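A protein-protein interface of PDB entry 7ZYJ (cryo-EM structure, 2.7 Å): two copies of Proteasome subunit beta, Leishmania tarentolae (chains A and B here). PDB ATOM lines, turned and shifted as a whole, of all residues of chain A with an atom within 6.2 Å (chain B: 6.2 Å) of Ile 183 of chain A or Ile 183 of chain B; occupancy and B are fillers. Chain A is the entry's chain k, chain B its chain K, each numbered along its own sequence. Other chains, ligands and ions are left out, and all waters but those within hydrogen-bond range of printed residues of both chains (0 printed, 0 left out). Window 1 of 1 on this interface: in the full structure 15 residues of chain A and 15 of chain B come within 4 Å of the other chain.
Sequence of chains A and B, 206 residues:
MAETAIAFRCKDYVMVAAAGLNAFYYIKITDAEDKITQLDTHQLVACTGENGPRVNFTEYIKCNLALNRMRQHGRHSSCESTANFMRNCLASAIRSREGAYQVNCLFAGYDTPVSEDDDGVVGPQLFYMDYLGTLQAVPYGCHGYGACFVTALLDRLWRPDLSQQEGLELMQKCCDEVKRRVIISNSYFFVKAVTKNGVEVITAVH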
ATOM      1  N   ALA A   2       7.763  23.406 -16.446  1.00  0.00           N
ATOM      2  CA  ALA A   2       7.640  23.314 -17.896  1.00  0.00           C
ATOM      3  C   ALA A   2       6.758  24.431 -18.437  1.00  0.00           C
ATOM      4  O   ALA A   2       7.046  25.011 -19.491  1.00  0.00           O
ATOM      5  CB  ALA A   2       7.083  21.946 -18.291  1.00  0.00           C
ATOM      6  N   LEU A  21      -0.205  24.586 -21.552  1.00  0.00           N
ATOM      7  CA  LEU A  21       0.358  23.278 -21.855  1.00  0.00           C
ATOM      8  C   LEU A  21      -0.092  22.219 -20.855  1.00  0.00           C
ATOM      9  O   LEU A  21      -0.141  22.461 -19.646  1.00  0.00           O
ATOM     10  CB  LEU A  21       1.883  23.356 -21.867  1.00  0.00           C
ATOM     11  CG  LEU A  21       2.631  22.050 -22.136  1.00  0.00           C
ATOM     12  CD1 LEU A  21       2.319  21.521 -23.522  1.00  0.00           C
ATOM     13  CD2 LEU A  21       4.116  22.257 -21.959  1.00  0.00           C
ATOM     14  N   ALA A  23       0.767  17.903 -20.600  1.00  0.00           N
ATOM     15  CA  ALA A  23       1.525  16.852 -21.282  1.00  0.00           C
ATOM     16  C   ALA A  23       1.599  15.559 -20.494  1.00  0.00           C
ATOM     17  O   ALA A  23       1.533  15.617 -19.275  1.00  0.00           O
ATOM     18  CB  ALA A  23       2.907  17.382 -21.488  1.00  0.00           C
ATOM     19  N   TYR A  25       4.349  12.992 -20.329  1.00  0.00           N
ATOM     20  CA  TYR A  25       5.725  12.759 -20.826  1.00  0.00           C
ATOM     21  C   TYR A  25       5.986  13.742 -21.965  1.00  0.00           C
ATOM     22  O   TYR A  25       5.865  14.944 -21.713  1.00  0.00           O
ATOM     23  CB  TYR A  25       5.934  11.272 -21.088  1.00  0.00           C
ATOM     24  CG  TYR A  25       6.040  10.533 -19.782  1.00  0.00           C
ATOM     25  CD1 TYR A  25       7.220  10.537 -19.061  1.00  0.00           C
ATOM     26  CD2 TYR A  25       4.935   9.930 -19.213  1.00  0.00           C
ATOM     27  CE1 TYR A  25       7.316   9.904 -17.834  1.00  0.00           C
ATOM     28  CE2 TYR A  25       5.009   9.292 -17.987  1.00  0.00           C
ATOM     29  CZ  TYR A  25       6.206   9.278 -17.297  1.00  0.00           C
ATOM     30  OH  TYR A  25       6.299   8.650 -16.089  1.00  0.00           O
ATOM     31  N   TYR A  26       6.321  13.256 -23.154  1.00  0.00           N
ATOM     32  CA  TYR A  26       6.682  14.163 -24.268  1.00  0.00           C
ATOM     33  C   TYR A  26       5.456  14.465 -25.123  1.00  0.00           C
ATOM     34  O   TYR A  26       5.605  15.185 -26.113  1.00  0.00           O
ATOM     35  CB  TYR A  26       7.808  13.552 -25.106  1.00  0.00           C
ATOM     36  CG  TYR A  26       7.531  12.208 -25.726  1.00  0.00           C
ATOM     37  CD1 TYR A  26       6.833  12.104 -26.915  1.00  0.00           C
ATOM     38  CD2 TYR A  26       7.995  11.047 -25.140  1.00  0.00           C
ATOM     39  CE1 TYR A  26       6.587  10.875 -27.499  1.00  0.00           C
ATOM     40  CE2 TYR A  26       7.759   9.810 -25.710  1.00  0.00           C
ATOM     41  CZ  TYR A  26       7.054   9.726 -26.894  1.00  0.00           C
ATOM     42  OH  TYR A  26       6.812   8.512 -27.464  1.00  0.00           O
ATOM     43  N   ILE A  27       4.296  13.924 -24.763  1.00  0.00           N
ATOM     44  CA  ILE A  27       3.083  14.112 -25.608  1.00  0.00           C
ATOM     45  C   ILE A  27       2.301  15.329 -25.135  1.00  0.00           C
ATOM     46  O   ILE A  27       2.001  15.401 -23.947  1.00  0.00           O
ATOM     47  CB  ILE A  27       2.205  12.850 -25.651  1.00  0.00           C
ATOM     48  CG1 ILE A  27       2.970  11.646 -26.201  1.00  0.00           C
ATOM     49  CG2 ILE A  27       0.925  13.116 -26.426  1.00  0.00           C
ATOM     50  CD1 ILE A  27       3.041  10.478 -25.252  1.00  0.00           C
ATOM     51  N   LYS A  28       2.017  16.253 -26.041  1.00  0.00           N
ATOM     52  CA  LYS A  28       1.176  17.409 -25.753  1.00  0.00           C
ATOM     53  C   LYS A  28      -0.279  16.960 -25.721  1.00  0.00           C
ATOM     54  O   LYS A  28      -0.894  16.750 -26.772  1.00  0.00           O
ATOM     55  CB  LYS A  28       1.398  18.499 -26.796  1.00  0.00           C
ATOM     56  CG  LYS A  28       0.624  19.780 -26.540  1.00  0.00           C
ATOM     57  CD  LYS A  28       1.428  21.008 -26.939  1.00  0.00           C
ATOM     58  CE  LYS A  28       2.173  20.796 -28.244  1.00  0.00           C
ATOM     59  NZ  LYS A  28       2.661  22.079 -28.817  1.00  0.00           N
ATOM     60  N   TYR A 145      10.318  27.633 -16.908  1.00  0.00           N
ATOM     61  CA  TYR A 145      11.620  27.664 -17.565  1.00  0.00           C
ATOM     62  C   TYR A 145      11.915  29.034 -18.157  1.00  0.00           C
ATOM     63  O   TYR A 145      13.044  29.529 -18.060  1.00  0.00           O
ATOM     64  CB  TYR A 145      11.682  26.591 -18.649  1.00  0.00           C
ATOM     65  CG  TYR A 145      11.890  25.194 -18.118  1.00  0.00           C
ATOM     66  CD1 TYR A 145      12.727  24.961 -17.036  1.00  0.00           C
ATOM     67  CD2 TYR A 145      11.249  24.109 -18.695  1.00  0.00           C
ATOM     68  CE1 TYR A 145      12.924  23.686 -16.551  1.00  0.00           C
ATOM     69  CE2 TYR A 145      11.435  22.831 -18.214  1.00  0.00           C
ATOM     70  CZ  TYR A 145      12.273  22.626 -17.140  1.00  0.00           C
ATOM     71  OH  TYR A 145      12.462  21.353 -16.657  1.00  0.00           O
ATOM     72  N   VAL A 178       9.454  33.785 -24.455  1.00  0.00           N
ATOM     73  CA  VAL A 178       9.321  32.431 -23.922  1.00  0.00           C
ATOM     74  C   VAL A 178       9.237  31.419 -25.059  1.00  0.00           C
ATOM     75  O   VAL A 178       9.885  30.367 -25.026  1.00  0.00           O
ATOM     76  CB  VAL A 178       8.099  32.324 -22.991  1.00  0.00           C
ATOM     77  CG1 VAL A 178       7.903  30.882 -22.552  1.00  0.00           C
ATOM     78  CG2 VAL A 178       8.274  33.214 -21.790  1.00  0.00           C
ATOM     79  N   ARG A 181      12.895  31.087 -26.688  1.00  0.00           N
ATOM     80  CA  ARG A 181      14.076  30.604 -25.985  1.00  0.00           C
ATOM     81  C   ARG A 181      13.876  29.309 -25.208  1.00  0.00           C
ATOM     82  O   ARG A 181      14.869  28.725 -24.761  1.00  0.00           O
ATOM     83  CB  ARG A 181      14.600  31.683 -25.027  1.00  0.00           C
ATOM     84  CG  ARG A 181      15.573  32.645 -25.681  1.00  0.00           C
ATOM     85  CD  ARG A 181      16.650  31.903 -26.450  1.00  0.00           C
ATOM     86  NE  ARG A 181      17.256  32.741 -27.477  1.00  0.00           N
ATOM     87  CZ  ARG A 181      18.080  32.298 -28.416  1.00  0.00           C
ATOM     88  NH1 ARG A 181      18.423  31.024 -28.489  1.00  0.00           N
ATOM     89  NH2 ARG A 181      18.570  33.155 -29.306  1.00  0.00           N
ATOM     90  N   VAL A 182      12.645  28.841 -25.029  1.00  0.00           N
ATOM     91  CA  VAL A 182      12.376  27.642 -24.241  1.00  0.00           C
ATOM     92  C   VAL A 182      12.123  26.476 -25.185  1.00  0.00           C
ATOM     93  O   VAL A 182      11.319  26.585 -26.120  1.00  0.00           O
ATOM     94  CB  VAL A 182      11.183  27.854 -23.294  1.00  0.00           C
ATOM     95  CG1 VAL A 182      10.963  26.622 -22.433  1.00  0.00           C
ATOM     96  CG2 VAL A 182      11.414  29.074 -22.425  1.00  0.00           C
ATOM     97  N   ILE A 183      12.813  25.356 -24.944  1.00  0.00           N
ATOM     98  CA  ILE A 183      12.625  24.176 -25.782  1.00  0.00           C
ATOM     99  C   ILE A 183      11.225  23.607 -25.595  1.00  0.00           C
ATOM    100  O   ILE A 183      10.646  23.040 -26.529  1.00  0.00           O
ATOM    101  CB  ILE A 183      13.711  23.122 -25.487  1.00  0.00           C
ATOM    102  CG1 ILE A 183      13.548  21.908 -26.400  1.00  0.00           C
ATOM    103  CG2 ILE A 183      13.631  22.655 -24.051  1.00  0.00           C
ATOM    104  CD1 ILE A 183      14.606  20.850 -26.190  1.00  0.00           C
ATOM    105  N   ILE A 184      10.658  23.746 -24.401  1.00  0.00           N
ATOM    106  CA  ILE A 184       9.299  23.291 -24.142  1.00  0.00           C
ATOM    107  C   ILE A 184       8.330  24.202 -24.881  1.00  0.00           C
ATOM    108  O   ILE A 184       8.367  25.428 -24.723  1.00  0.00           O
ATOM    109  CB  ILE A 184       9.012  23.276 -22.632  1.00  0.00           C
ATOM    110  CG1 ILE A 184      10.029  22.391 -21.908  1.00  0.00           C
ATOM    111  CG2 ILE A 184       7.608  22.793 -22.363  1.00  0.00           C
ATOM    112  CD1 ILE A 184       9.885  20.918 -22.219  1.00  0.00           C
ATOM    113  N   SER A 185       7.459  23.605 -25.691  1.00  0.00           N
ATOM    114  CA  SER A 185       6.568  24.368 -26.560  1.00  0.00           C
ATOM    115  C   SER A 185       5.430  24.955 -25.736  1.00  0.00           C
ATOM    116  O   SER A 185       4.547  24.226 -25.271  1.00  0.00           O
ATOM    117  CB  SER A 185       6.030  23.483 -27.681  1.00  0.00           C
ATOM    118  OG  SER A 185       5.103  24.189 -28.485  1.00  0.00           O
ATOM    119  N   ASN A 186       5.448  26.272 -25.554  1.00  0.00           N
ATOM    120  CA  ASN A 186       4.355  27.011 -24.929  1.00  0.00           C
ATOM    121  C   ASN A 186       3.772  27.930 -26.001  1.00  0.00           C
ATOM    122  O   ASN A 186       4.147  29.097 -26.108  1.00  0.00           O
ATOM    123  CB  ASN A 186       4.846  27.797 -23.717  1.00  0.00           C
ATOM    124  CG  ASN A 186       5.207  26.903 -22.550  1.00  0.00           C
ATOM    125  OD1 ASN A 186       4.709  25.784 -22.430  1.00  0.00           O
ATOM    126  ND2 ASN A 186       6.081  27.392 -21.680  1.00  0.00           N
ATOM    127  N   ALA B   2      14.932  14.110 -29.143  1.00  0.00           N
ATOM    128  CA  ALA B   2      14.224  15.380 -29.021  1.00  0.00           C
ATOM    129  C   ALA B   2      13.910  15.957 -30.395  1.00  0.00           C
ATOM    130  O   ALA B   2      12.825  16.507 -30.619  1.00  0.00           O
ATOM    131  CB  ALA B   2      15.049  16.365 -28.194  1.00  0.00           C
ATOM    132  N   LEU B  21      16.511  21.986 -34.272  1.00  0.00           N
ATOM    133  CA  LEU B  21      16.641  22.312 -32.859  1.00  0.00           C
ATOM    134  C   LEU B  21      18.041  22.020 -32.333  1.00  0.00           C
ATOM    135  O   LEU B  21      18.644  20.993 -32.656  1.00  0.00           O
ATOM    136  CB  LEU B  21      15.615  21.526 -32.045  1.00  0.00           C
ATOM    137  CG  LEU B  21      15.644  21.730 -30.532  1.00  0.00           C
ATOM    138  CD1 LEU B  21      15.318  23.164 -30.168  1.00  0.00           C
ATOM    139  CD2 LEU B  21      14.688  20.772 -29.861  1.00  0.00           C
ATOM    140  N   ALA B  23      19.744  22.590 -28.299  1.00  0.00           N
ATOM    141  CA  ALA B  23      19.310  23.004 -26.973  1.00  0.00           C
ATOM    142  C   ALA B  23      20.395  22.744 -25.939  1.00  0.00           C
ATOM    143  O   ALA B  23      21.290  21.920 -26.140  1.00  0.00           O
ATOM    144  CB  ALA B  23      18.018  22.286 -26.561  1.00  0.00           C
ATOM    145  N   TYR B  25      19.666  21.885 -22.260  1.00  0.00           N
ATOM    146  CA  TYR B  25      19.006  21.349 -21.072  1.00  0.00           C
ATOM    147  C   TYR B  25      17.632  21.932 -20.758  1.00  0.00           C
ATOM    148  O   TYR B  25      16.821  21.254 -20.118  1.00  0.00           O
ATOM    149  CB  TYR B  25      19.902  21.565 -19.847  1.00  0.00           C
ATOM    150  CG  TYR B  25      20.896  20.461 -19.575  1.00  0.00           C
ATOM    151  CD1 TYR B  25      20.473  19.198 -19.184  1.00  0.00           C
ATOM    152  CD2 TYR B  25      22.261  20.689 -19.691  1.00  0.00           C
ATOM    153  CE1 TYR B  25      21.383  18.190 -18.930  1.00  0.00           C
ATOM    154  CE2 TYR B  25      23.175  19.690 -19.439  1.00  0.00           C
ATOM    155  CZ  TYR B  25      22.733  18.442 -19.059  1.00  0.00           C
ATOM    156  OH  TYR B  25      23.644  17.442 -18.806  1.00  0.00           O
ATOM    157  N   TYR B  26      17.337  23.162 -21.183  1.00  0.00           N
ATOM    158  CA  TYR B  26      15.969  23.553 -21.513  1.00  0.00           C
ATOM    159  C   TYR B  26      15.983  24.740 -22.467  1.00  0.00           C
ATOM    160  O   TYR B  26      14.927  25.262 -22.836  1.00  0.00           O
ATOM    161  CB  TYR B  26      15.131  23.859 -20.263  1.00  0.00           C
ATOM    162  CG  TYR B  26      15.668  24.904 -19.315  1.00  0.00           C
ATOM    163  CD1 TYR B  26      15.498  26.256 -19.577  1.00  0.00           C
ATOM    164  CD2 TYR B  26      16.302  24.540 -18.136  1.00  0.00           C
ATOM    165  CE1 TYR B  26      15.970  27.215 -18.707  1.00  0.00           C
ATOM    166  CE2 TYR B  26      16.778  25.493 -17.260  1.00  0.00           C
ATOM    167  CZ  TYR B  26      16.608  26.829 -17.551  1.00  0.00           C
ATOM    168  OH  TYR B  26      17.079  27.787 -16.684  1.00  0.00           O
ATOM    169  N   ILE B  27      17.174  25.186 -22.854  1.00  0.00           N
ATOM    170  CA  ILE B  27      17.355  26.460 -23.541  1.00  0.00           C
ATOM    171  C   ILE B  27      17.554  26.197 -25.023  1.00  0.00           C
ATOM    172  O   ILE B  27      18.449  25.440 -25.410  1.00  0.00           O
ATOM    173  CB  ILE B  27      18.549  27.238 -22.961  1.00  0.00           C
ATOM    174  CG1 ILE B  27      18.292  27.602 -21.499  1.00  0.00           C
ATOM    175  CG2 ILE B  27      18.824  28.484 -23.787  1.00  0.00           C
ATOM    176  CD1 ILE B  27      19.520  27.504 -20.626  1.00  0.00           C
ATOM    177  N   LYS B  28      16.739  26.842 -25.853  1.00  0.00           N
ATOM    178  CA  LYS B  28      16.858  26.710 -27.299  1.00  0.00           C
ATOM    179  C   LYS B  28      18.037  27.550 -27.773  1.00  0.00           C
ATOM    180  O   LYS B  28      17.934  28.777 -27.873  1.00  0.00           O
ATOM    181  CB  LYS B  28      15.562  27.144 -27.978  1.00  0.00           C
ATOM    182  CG  LYS B  28      15.555  26.969 -29.487  1.00  0.00           C
ATOM    183  CD  LYS B  28      14.185  26.544 -29.995  1.00  0.00           C
ATOM    184  CE  LYS B  28      13.065  27.289 -29.292  1.00  0.00           C
ATOM    185  NZ  LYS B  28      11.772  27.149 -30.011  1.00  0.00           N
ATOM    186  N   TYR B 145      10.876  12.001 -31.072  1.00  0.00           N
ATOM    187  CA  TYR B 145       9.645  11.869 -30.300  1.00  0.00           C
ATOM    188  C   TYR B 145       8.421  11.817 -31.205  1.00  0.00           C
ATOM    189  O   TYR B 145       7.502  11.026 -30.969  1.00  0.00           O
ATOM    190  CB  TYR B 145       9.526  13.023 -29.308  1.00  0.00           C
ATOM    191  CG  TYR B 145      10.406  12.877 -28.092  1.00  0.00           C
ATOM    192  CD1 TYR B 145      10.608  11.638 -27.502  1.00  0.00           C
ATOM    193  CD2 TYR B 145      11.039  13.979 -27.535  1.00  0.00           C
ATOM    194  CE1 TYR B 145      11.409  11.501 -26.388  1.00  0.00           C
ATOM    195  CE2 TYR B 145      11.845  13.850 -26.423  1.00  0.00           C
ATOM    196  CZ  TYR B 145      12.027  12.610 -25.855  1.00  0.00           C
ATOM    197  OH  TYR B 145      12.829  12.478 -24.747  1.00  0.00           O
ATOM    198  N   VAL B 178       3.971  16.878 -35.995  1.00  0.00           N
ATOM    199  CA  VAL B 178       5.051  16.889 -35.009  1.00  0.00           C
ATOM    200  C   VAL B 178       4.966  18.139 -34.143  1.00  0.00           C
ATOM    201  O   VAL B 178       5.103  18.078 -32.916  1.00  0.00           O
ATOM    202  CB  VAL B 178       6.424  16.780 -35.697  1.00  0.00           C
ATOM    203  CG1 VAL B 178       7.535  16.924 -34.668  1.00  0.00           C
ATOM    204  CG2 VAL B 178       6.550  15.464 -36.416  1.00  0.00           C
ATOM    205  N   ARG B 181       1.849  17.702 -31.644  1.00  0.00           N
ATOM    206  CA  ARG B 181       1.741  16.665 -30.627  1.00  0.00           C
ATOM    207  C   ARG B 181       2.973  16.494 -29.748  1.00  0.00           C
ATOM    208  O   ARG B 181       2.888  15.789 -28.737  1.00  0.00           O
ATOM    209  CB  ARG B 181       1.406  15.317 -31.281  1.00  0.00           C
ATOM    210  CG  ARG B 181      -0.083  15.085 -31.455  1.00  0.00           C
ATOM    211  CD  ARG B 181      -0.839  15.376 -30.170  1.00  0.00           C
ATOM    212  NE  ARG B 181      -2.243  15.670 -30.426  1.00  0.00           N
ATOM    213  CZ  ARG B 181      -3.087  16.140 -29.518  1.00  0.00           C
ATOM    214  NH1 ARG B 181      -2.702  16.379 -28.276  1.00  0.00           N
ATOM    215  NH2 ARG B 181      -4.349  16.377 -29.865  1.00  0.00           N
ATOM    216  N   VAL B 182       4.103  17.105 -30.087  1.00  0.00           N
ATOM    217  CA  VAL B 182       5.338  16.934 -29.328  1.00  0.00           C
ATOM    218  C   VAL B 182       5.551  18.156 -28.447  1.00  0.00           C
ATOM    219  O   VAL B 182       5.475  19.296 -28.925  1.00  0.00           O
ATOM    220  CB  VAL B 182       6.540  16.709 -30.260  1.00  0.00           C
ATOM    221  CG1 VAL B 182       7.803  16.465 -29.450  1.00  0.00           C
ATOM    222  CG2 VAL B 182       6.271  15.540 -31.188  1.00  0.00           C
ATOM    223  N   ILE B 183       5.815  17.922 -27.158  1.00  0.00           N
ATOM    224  CA  ILE B 183       6.053  19.030 -26.239  1.00  0.00           C
ATOM    225  C   ILE B 183       7.349  19.746 -26.593  1.00  0.00           C
ATOM    226  O   ILE B 183       7.472  20.960 -26.391  1.00  0.00           O
ATOM    227  CB  ILE B 183       6.061  18.533 -24.779  1.00  0.00           C
ATOM    228  CG1 ILE B 183       6.258  19.698 -23.811  1.00  0.00           C
ATOM    229  CG2 ILE B 183       7.174  17.533 -24.557  1.00  0.00           C
ATOM    230  CD1 ILE B 183       6.236  19.285 -22.358  1.00  0.00           C
ATOM    231  N   ILE B 184       8.328  19.023 -27.126  1.00  0.00           N
ATOM    232  CA  ILE B 184       9.582  19.629 -27.555  1.00  0.00           C
ATOM    233  C   ILE B 184       9.316  20.470 -28.796  1.00  0.00           C
ATOM    234  O   ILE B 184       8.760  19.980 -29.786  1.00  0.00           O
ATOM    235  CB  ILE B 184      10.639  18.549 -27.826  1.00  0.00           C
ATOM    236  CG1 ILE B 184      10.851  17.689 -26.579  1.00  0.00           C
ATOM    237  CG2 ILE B 184      11.942  19.178 -28.260  1.00  0.00           C
ATOM    238  CD1 ILE B 184      11.513  18.425 -25.438  1.00  0.00           C
ATOM    239  N   SER B 185       9.713  21.738 -28.746  1.00  0.00           N
ATOM    240  CA  SER B 185       9.400  22.686 -29.811  1.00  0.00           C
ATOM    241  C   SER B 185      10.306  22.429 -31.008  1.00  0.00           C
ATOM    242  O   SER B 185      11.509  22.701 -30.956  1.00  0.00           O
ATOM    243  CB  SER B 185       9.552  24.120 -29.310  1.00  0.00           C
ATOM    244  OG  SER B 185       9.326  25.050 -30.356  1.00  0.00           O
ATOM    245  N   ASN B 186       9.729  21.905 -32.084  1.00  0.00           N
ATOM    246  CA  ASN B 186      10.414  21.744 -33.364  1.00  0.00           C
ATOM    247  C   ASN B 186       9.710  22.659 -34.363  1.00  0.00           C
ATOM    248  O   ASN B 186       8.815  22.232 -35.091  1.00  0.00           O
ATOM    249  CB  ASN B 186      10.395  20.289 -33.819  1.00  0.00           C
ATOM    250  CG  ASN B 186      11.286  19.401 -32.974  1.00  0.00           C
ATOM    251  OD1 ASN B 186      12.243  19.867 -32.360  1.00  0.00           O
ATOM    252  ND2 ASN B 186      10.974  18.113 -32.941  1.00  0.00           N
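The backbone carbonyl oxygen (O) of Tyr 26 of chain B lies within hydrogen-bond range of the backbone NH (N) of Ile 183 of chain A (3.0 Å). The backbone NH (N) of Lys 28 of chain B sits at hydrogen-bond distance from the backbone carbonyl oxygen (O) of Arg 181 of chain A (2.9 Å). O of Arg 181 of chain B lies within hydrogen-bond range of N of Lys 28 of chain A (2.9 Å). The backbone carbonyl oxygen (O) of Tyr 26 of chain A lies within hydrogen-bond range of the backbone NH (N) of Ile 183 of chain B. The backbone NH (N) of Ser 185 of chain A is in hydrogen-bond range of the backbone carbonyl oxygen (O) of Ile 183 of chain B. The backbone NH of Ser 185 of chain B sits at hydrogen-bond distance from the backbone carbonyl oxygen of Ile 183 of chain A, 2.7 Å away.
The side-chain amino group (NZ) of Lys 28 of chain B is in hydrogen-bond range of the side-chain hydroxyl (OG) of Ser 185 of chain B, at 3.2 Å. The side-chain amino group (NZ) of Lys 28 of chain A lies within hydrogen-bond range of the side-chain hydroxyl (OG) of Ser 185 of chain A (3.2 Å).
Among the printed residues, pairs that only touch across the chains: Leu 21 of chain A with Ile 183 of chain B (3.7 Å), Ala 23 of chain A with Ile 183 of chain B (3.9 Å), Tyr 26 of chain A with Tyr 145 of chain B (3.6 Å), Tyr 26 of chain A with Arg 181 of chain B (3.8 Å), Tyr 26 of chain A with Val 182 of chain B (3.7 Å), Ile 27 of chain A with Arg 181 of chain B (3.6 Å), Lys 28 of chain A with Val 182 of chain B (3.7 Å), Tyr 145 of chain A with Tyr 26 of chain B (3.7 Å), Arg 181 of chain A with Tyr 26 of chain B (3.96 Å), Arg 181 of chain A with Ile 27 of chain B (3.6 Å), Val 182 of chain A with Tyr 26 of chain B (3.8 Å), Val 182 of chain A with Lys 28 of chain B (3.7 Å), Ile 183 of chain A with Leu 21 of chain B (3.7 Å), Ile 183 of chain A with Ala 23 of chain B (3.7 Å), Ile 183 of chain A with Ile 183 of chain B (3.8 Å), Ile 183 of chain A with Ile 184 of chain B (3.7 Å), Ile 184 of chain A with Ile 183 of chain B (3.7 Å) and Ser 185 of chain A with Ser 185 of chain B (3.9 Å).
Printed residues of chain A within 4 Å of Ile 183 of chain B: Leu 21, Ala 23, Tyr 26, Ile 183, Ile 184 and Ser 185. Of the printed residues of chain A, Ile 27 of chain B touches Arg 181 (3.6 Å). Printed residues of chain A within 4 Å of Lys 28 of chain B: Arg 181 and Val 182. Of the printed residues of chain B, Ile 184 of chain A touches Ile 183. Printed residues of chain B within 4 Å of Ala 23 of chain A: Ile 183 (3.9 Å). Of the printed residues of chain B, Tyr 145 of chain A touches Tyr 26 (3.7 Å). Tyr 25 of chain B touches none of the printed residues of chain A. The nearest residue of chain B that does not touch Ile 183 of chain A is Lys 28 of chain B (4.3 Å).
Of the 15 printed residues of chain A, 11 touch a printed residue of chain B. Printed residues of chain A that touch a printed residue of chain B: Leu 21, Ala 23, Tyr 26, Ile 27, Lys 28, Tyr 145, Arg 181, Val 182, Ile 183, Ile 184 and Ser 185. Printed residues of chain B that touch a printed residue of chain A: Leu 21, Ala 23, Tyr 26, Ile 27, Lys 28, Tyr 145, Arg 181, Val 182, Ile 183, Ile 184 and Ser 185. Hydrophobic or aromatic side chains of chain B within 4 Å of the printed part of chain A: Leu 21, Ala 23, Tyr 26, Tyr 145, Ile 183 and Ile 184. Along chain B the printed residues that touch a printed residue of chain A span positions 21 to 185. Among the printed residues, no Asp or Glu carboxylate lies within 4 Å of a Lys or Arg side-chain nitrogen of the other chain.
Tyr 26 of chain A touches Tyr 145 of chain B, and with the chains exchanged Tyr 145 of chain A touches Tyr 26 of chain B. Ile 27 of chain A touches Arg 181 of chain B, and with the chains exchanged Arg 181 of chain A touches Ile 27 of chain B. Lys 28 of chain A touches Arg 181 of chain B, and with the chains exchanged Arg 181 of chain A touches Lys 28 of chain B. Ser 185 of chain A touches its own counterpart, Ser 185 of chain B.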
